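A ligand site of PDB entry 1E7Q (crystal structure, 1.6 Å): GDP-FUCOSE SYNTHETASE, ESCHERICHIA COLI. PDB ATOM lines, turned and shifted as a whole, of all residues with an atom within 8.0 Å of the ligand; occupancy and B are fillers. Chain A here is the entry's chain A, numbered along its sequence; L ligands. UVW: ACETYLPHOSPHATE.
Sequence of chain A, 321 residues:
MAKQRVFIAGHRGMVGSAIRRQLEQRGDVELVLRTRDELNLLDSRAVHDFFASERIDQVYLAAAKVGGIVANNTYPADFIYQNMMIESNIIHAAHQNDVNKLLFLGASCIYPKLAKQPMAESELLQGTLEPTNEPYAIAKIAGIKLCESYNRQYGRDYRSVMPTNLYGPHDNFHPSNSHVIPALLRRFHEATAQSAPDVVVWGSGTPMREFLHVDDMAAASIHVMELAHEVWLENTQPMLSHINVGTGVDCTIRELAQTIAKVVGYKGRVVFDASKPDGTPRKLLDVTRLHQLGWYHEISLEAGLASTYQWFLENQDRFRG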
ATOM      1  N   LYS A  65      -3.786 -14.041   3.721  1.00  0.00           N
ATOM      2  CA  LYS A  65      -3.669 -15.530   3.790  1.00  0.00           C
ATOM      3  C   LYS A  65      -4.955 -16.038   4.429  1.00  0.00           C
ATOM      4  O   LYS A  65      -5.354 -15.666   5.527  1.00  0.00           O
ATOM      5  CB  LYS A  65      -2.448 -15.802   4.676  1.00  0.00           C
ATOM      6  CG  LYS A  65      -2.260 -17.228   5.133  1.00  0.00           C
ATOM      7  CD  LYS A  65      -2.164 -18.156   3.978  1.00  0.00           C
ATOM      8  CE  LYS A  65      -1.670 -19.514   4.515  1.00  0.00           C
ATOM      9  NZ  LYS A  65      -1.568 -20.373   3.296  1.00  0.00           N
ATOM     10  N   VAL A  66      -5.750 -16.725   3.568  1.00  0.00           N
ATOM     11  CA  VAL A  66      -7.120 -17.125   3.888  1.00  0.00           C
ATOM     12  C   VAL A  66      -7.236 -18.638   3.662  1.00  0.00           C
ATOM     13  O   VAL A  66      -6.578 -19.171   2.717  1.00  0.00           O
ATOM     14  CB  VAL A  66      -8.093 -16.400   2.927  1.00  0.00           C
ATOM     15  CG1 VAL A  66      -9.524 -16.683   3.135  1.00  0.00           C
ATOM     16  CG2 VAL A  66      -7.847 -14.913   3.036  1.00  0.00           C
ATOM     17  N   GLY A  67      -8.031 -19.264   4.511  1.00  0.00           N
ATOM     18  CA  GLY A  67      -8.255 -20.711   4.321  1.00  0.00           C
ATOM     19  C   GLY A  67      -9.498 -21.119   5.128  1.00  0.00           C
ATOM     20  O   GLY A  67     -10.186 -20.317   5.794  1.00  0.00           O
ATOM     21  N   GLY A  68      -9.765 -22.411   5.135  1.00  0.00           N
ATOM     22  CA  GLY A  68     -10.863 -23.013   5.810  1.00  0.00           C
ATOM     23  C   GLY A  68     -10.503 -23.574   7.162  1.00  0.00           C
ATOM     24  O   GLY A  68      -9.511 -23.173   7.803  1.00  0.00           O
ATOM     25  N   ILE A  69     -11.337 -24.475   7.708  1.00  0.00           N
ATOM     26  CA  ILE A  69     -11.236 -24.908   9.072  1.00  0.00           C
ATOM     27  C   ILE A  69      -9.926 -25.660   9.339  1.00  0.00           C
ATOM     28  O   ILE A  69      -9.244 -25.474  10.350  1.00  0.00           O
ATOM     29  CB  ILE A  69     -12.456 -25.577   9.630  1.00  0.00           C
ATOM     30  CG1 ILE A  69     -12.851 -26.894   9.039  1.00  0.00           C
ATOM     31  CG2 ILE A  69     -13.695 -24.686   9.666  1.00  0.00           C
ATOM     32  CD1 ILE A  69     -14.219 -27.377   9.535  1.00  0.00           C
ATOM     33  N   VAL A  70      -9.628 -26.613   8.424  1.00  0.00           N
ATOM     34  CA  VAL A  70      -8.419 -27.379   8.599  1.00  0.00           C
ATOM     35  C   VAL A  70      -7.200 -26.473   8.506  1.00  0.00           C
ATOM     36  O   VAL A  70      -6.302 -26.535   9.384  1.00  0.00           O
ATOM     37  CB  VAL A  70      -8.343 -28.514   7.561  1.00  0.00           C
ATOM     38  CG1 VAL A  70      -6.959 -29.154   7.608  1.00  0.00           C
ATOM     39  CG2 VAL A  70      -9.439 -29.533   7.733  1.00  0.00           C
ATOM     40  N   ALA A  71      -7.206 -25.559   7.533  1.00  0.00           N
ATOM     41  CA  ALA A  71      -6.002 -24.718   7.336  1.00  0.00           C
ATOM     42  C   ALA A  71      -5.786 -23.876   8.598  1.00  0.00           C
ATOM     43  O   ALA A  71      -4.641 -23.685   9.010  1.00  0.00           O
ATOM     44  CB  ALA A  71      -6.155 -23.873   6.074  1.00  0.00           C
ATOM     45  N   ASN A  72      -6.851 -23.183   9.041  1.00  0.00           N
ATOM     46  CA  ASN A  72      -6.669 -22.254  10.154  1.00  0.00           C
ATOM     47  C   ASN A  72      -6.187 -23.000  11.412  1.00  0.00           C
ATOM     48  O   ASN A  72      -5.518 -22.386  12.253  1.00  0.00           O
ATOM     49  CB  ASN A  72      -8.000 -21.537  10.491  1.00  0.00           C
ATOM     50  CG  ASN A  72      -8.120 -20.274   9.607  1.00  0.00           C
ATOM     51  OD1 ASN A  72      -7.683 -19.217  10.047  1.00  0.00           O
ATOM     52  ND2 ASN A  72      -8.687 -20.355   8.435  1.00  0.00           N
ATOM     53  N   ASN A  73      -6.607 -24.262  11.610  1.00  0.00           N
ATOM     54  CA  ASN A  73      -6.149 -24.980  12.806  1.00  0.00           C
ATOM     55  C   ASN A  73      -4.797 -25.636  12.580  1.00  0.00           C
ATOM     56  O   ASN A  73      -4.096 -25.832  13.587  1.00  0.00           O
ATOM     57  CB  ASN A  73      -7.140 -26.115  13.151  1.00  0.00           C
ATOM     58  CG  ASN A  73      -8.333 -25.606  13.931  1.00  0.00           C
ATOM     59  OD1 ASN A  73      -8.262 -25.165  15.077  1.00  0.00           O
ATOM     60  ND2 ASN A  73      -9.505 -25.768  13.350  1.00  0.00           N
ATOM     61  N   THR A  74      -4.399 -25.826  11.329  1.00  0.00           N
ATOM     62  CA  THR A  74      -3.136 -26.554  11.068  1.00  0.00           C
ATOM     63  C   THR A  74      -1.952 -25.622  10.947  1.00  0.00           C
ATOM     64  O   THR A  74      -0.836 -25.947  11.381  1.00  0.00           O
ATOM     65  CB  THR A  74      -3.350 -27.364   9.780  1.00  0.00           C
ATOM     66  OG1 THR A  74      -4.389 -28.330  10.043  1.00  0.00           O
ATOM     67  CG2 THR A  74      -2.089 -28.046   9.352  1.00  0.00           C
ATOM     68  N   TYR A  75      -2.189 -24.419  10.442  1.00  0.00           N
ATOM     69  CA  TYR A  75      -1.120 -23.436  10.260  1.00  0.00           C
ATOM     70  C   TYR A  75      -1.436 -22.104  10.970  1.00  0.00           C
ATOM     71  O   TYR A  75      -1.379 -21.033  10.344  1.00  0.00           O
ATOM     72  CB  TYR A  75      -1.030 -23.177   8.726  1.00  0.00           C
ATOM     73  CG  TYR A  75      -0.839 -24.409   7.863  1.00  0.00           C
ATOM     74  CD1 TYR A  75       0.383 -25.046   7.875  1.00  0.00           C
ATOM     75  CD2 TYR A  75      -1.884 -25.031   7.221  1.00  0.00           C
ATOM     76  CE1 TYR A  75       0.598 -26.189   7.134  1.00  0.00           C
ATOM     77  CE2 TYR A  75      -1.679 -26.171   6.449  1.00  0.00           C
ATOM     78  CZ  TYR A  75      -0.436 -26.768   6.464  1.00  0.00           C
ATOM     79  OH  TYR A  75      -0.193 -27.939   5.756  1.00  0.00           O
ATOM     80  N   PHE A  79      -1.267 -17.955   9.570  1.00  0.00           N
ATOM     81  CA  PHE A  79      -2.427 -17.055   9.423  1.00  0.00           C
ATOM     82  C   PHE A  79      -2.329 -15.762  10.253  1.00  0.00           C
ATOM     83  O   PHE A  79      -2.708 -14.694   9.779  1.00  0.00           O
ATOM     84  CB  PHE A  79      -3.723 -17.803   9.824  1.00  0.00           C
ATOM     85  CG  PHE A  79      -4.231 -18.626   8.694  1.00  0.00           C
ATOM     86  CD1 PHE A  79      -5.031 -18.078   7.711  1.00  0.00           C
ATOM     87  CD2 PHE A  79      -3.799 -19.953   8.581  1.00  0.00           C
ATOM     88  CE1 PHE A  79      -5.484 -18.835   6.639  1.00  0.00           C
ATOM     89  CE2 PHE A  79      -4.246 -20.700   7.483  1.00  0.00           C
ATOM     90  CZ  PHE A  79      -5.116 -20.186   6.552  1.00  0.00           C
ATOM     91  N   THR A 132     -10.967 -21.904  16.275  1.00  0.00           N
ATOM     92  CA  THR A 132     -10.400 -22.277  14.961  1.00  0.00           C
ATOM     93  C   THR A 132      -9.869 -20.995  14.299  1.00  0.00           C
ATOM     94  O   THR A 132      -8.857 -21.147  13.638  1.00  0.00           O
ATOM     95  CB  THR A 132     -11.511 -22.875  14.094  1.00  0.00           C
ATOM     96  OG1 THR A 132     -11.728 -24.204  14.579  1.00  0.00           O
ATOM     97  CG2 THR A 132     -11.300 -22.789  12.624  1.00  0.00           C
ATOM     98  N   ASN A 172     -13.162 -21.783  -4.291  1.00  0.00           N
ATOM     99  CA  ASN A 172     -12.553 -23.107  -4.364  1.00  0.00           C
ATOM    100  C   ASN A 172     -13.615 -24.197  -4.351  1.00  0.00           C
ATOM    101  O   ASN A 172     -14.119 -24.591  -3.287  1.00  0.00           O
ATOM    102  CB  ASN A 172     -11.601 -23.326  -3.169  1.00  0.00           C
ATOM    103  CG  ASN A 172     -11.093 -24.765  -3.165  1.00  0.00           C
ATOM    104  OD1 ASN A 172     -10.578 -25.287  -2.177  1.00  0.00           O
ATOM    105  ND2 ASN A 172     -11.174 -25.439  -4.324  1.00  0.00           N
ATOM    106  N   HIS A 174     -14.217 -27.438  -4.330  1.00  0.00           N
ATOM    107  CA  HIS A 174     -13.681 -28.785  -4.027  1.00  0.00           C
ATOM    108  C   HIS A 174     -14.585 -29.343  -2.933  1.00  0.00           C
ATOM    109  O   HIS A 174     -15.042 -28.557  -2.087  1.00  0.00           O
ATOM    110  CB  HIS A 174     -12.235 -28.699  -3.563  1.00  0.00           C
ATOM    111  CG  HIS A 174     -11.685 -30.044  -3.187  1.00  0.00           C
ATOM    112  ND1 HIS A 174     -12.103 -30.733  -2.066  1.00  0.00           N
ATOM    113  CD2 HIS A 174     -10.696 -30.784  -3.731  1.00  0.00           C
ATOM    114  CE1 HIS A 174     -11.411 -31.856  -1.964  1.00  0.00           C
ATOM    115  NE2 HIS A 174     -10.555 -31.916  -2.963  1.00  0.00           N
ATOM    116  N   SER A 176     -14.173 -30.989  -0.443  1.00  0.00           N
ATOM    117  CA  SER A 176     -13.858 -31.024   0.994  1.00  0.00           C
ATOM    118  C   SER A 176     -13.579 -29.629   1.511  1.00  0.00           C
ATOM    119  O   SER A 176     -13.327 -29.545   2.729  1.00  0.00           O
ATOM    120  CB  SER A 176     -12.784 -32.086   1.194  1.00  0.00           C
ATOM    121  OG  SER A 176     -13.261 -33.444   0.894  1.00  0.00           O
ATOM    122  N   ASN A 177     -13.942 -28.566   0.747  1.00  0.00           N
ATOM    123  CA  ASN A 177     -13.846 -27.212   1.293  1.00  0.00           C
ATOM    124  C   ASN A 177     -14.772 -27.060   2.491  1.00  0.00           C
ATOM    125  O   ASN A 177     -15.902 -27.558   2.433  1.00  0.00           O
ATOM    126  CB  ASN A 177     -14.255 -26.190   0.214  1.00  0.00           C
ATOM    127  CG  ASN A 177     -14.107 -24.741   0.560  1.00  0.00           C
ATOM    128  OD1 ASN A 177     -13.913 -24.272   1.676  1.00  0.00           O
ATOM    129  ND2 ASN A 177     -13.977 -23.924  -0.487  1.00  0.00           N
ATOM    130  N   SER A 178     -14.307 -26.405   3.542  1.00  0.00           N
ATOM    131  CA  SER A 178     -15.163 -26.283   4.710  1.00  0.00           C
ATOM    132  C   SER A 178     -16.228 -25.210   4.508  1.00  0.00           C
ATOM    133  O   SER A 178     -17.170 -25.116   5.290  1.00  0.00           O
ATOM    134  CB  SER A 178     -14.313 -26.051   5.982  1.00  0.00           C
ATOM    135  OG  SER A 178     -13.598 -24.854   5.818  1.00  0.00           O
ATOM    136  N   HIS A 179     -16.061 -24.364   3.486  1.00  0.00           N
ATOM    137  CA  HIS A 179     -17.081 -23.357   3.160  1.00  0.00           C
ATOM    138  C   HIS A 179     -18.290 -23.998   2.459  1.00  0.00           C
ATOM    139  O   HIS A 179     -18.090 -24.639   1.423  1.00  0.00           O
ATOM    140  CB  HIS A 179     -16.479 -22.267   2.331  1.00  0.00           C
ATOM    141  CG  HIS A 179     -15.416 -21.466   3.036  1.00  0.00           C
ATOM    142  ND1 HIS A 179     -14.073 -21.599   2.754  1.00  0.00           N
ATOM    143  CD2 HIS A 179     -15.525 -20.576   4.044  1.00  0.00           C
ATOM    144  CE1 HIS A 179     -13.397 -20.807   3.556  1.00  0.00           C
ATOM    145  NE2 HIS A 179     -14.255 -20.167   4.331  1.00  0.00           N
HETATM  146  C1  UVW L   1      -8.406 -25.388   3.953  1.00  0.00           C
HETATM  147  O1  UVW L   1      -8.186 -24.279   3.148  1.00  0.00           O
HETATM  148  C1M UVW L   1      -7.524 -26.435   3.558  1.00  0.00           C
HETATM  149  O2  UVW L   1      -9.338 -25.463   5.233  1.00  0.00           O
HETATM  150  P   UVW L   1     -10.348 -26.470   4.834  1.00  0.00           P
HETATM  151  O1P UVW L   1     -11.174 -26.917   5.922  1.00  0.00           O
HETATM  152  O2P UVW L   1     -11.247 -25.703   3.986  1.00  0.00           O
HETATM  153  O3P UVW L   1      -9.860 -27.630   3.882  1.00  0.00           O
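O of Val 70 lies within hydrogen-bond range of OG1 of Thr 74 (2.7 Å).
O of Ile 69 sits at hydrogen-bond distance from ND2 of Asn 73 (3.0 Å).
The backbone NH of Ile 69 sits at hydrogen-bond distance from the side-chain hydroxyl of Ser 178 (3.0 Å).
O of Gly 68 is in hydrogen-bond range of ND2 of Asn 72 (3.0 Å).
The backbone NH (N) of His 179 sits at hydrogen-bond distance from the side-chain amide oxygen (OD1) of Asn 177 (2.8 Å).
The backbone carbonyl oxygen of Asn 172 sits at hydrogen-bond distance from the side-chain amide nitrogen of Asn 177, 2.9 Å away.
O of Gly 67 lies within hydrogen-bond range of ND2 of Asn 72 (3.0 Å).
Gly 67 touches the ligand.
Asn 177 touches the ligand (OD1 to O2P, 3.8 Å).
Hydrophobic or aromatic side chains that line the ligand: Ile 69, Val 70 and Ala 71.
Within 4 Å of the ligand: Gly 67, Gly 68, Ile 69, Val 70, Ala 71, Asn 177 and Ser 178.
N of Ser 178 is in hydrogen-bond range of O2P of the ligand (3.2 Å).
O1P of the ligand is in hydrogen-bond range of N of Val 70, at 3.0 Å.
N of Ile 69 lies within hydrogen-bond range of O1P of the ligand (3.0 Å).
O2P of the ligand sits at hydrogen-bond distance from OG of Ser 178 (3.1 Å).
N of Ala 71 is in hydrogen-bond range of O2 of the ligand (3.1 Å).
The backbone NH of Gly 68 lies close to an oxygen (O2) of the ligand, at 3.1 Å.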
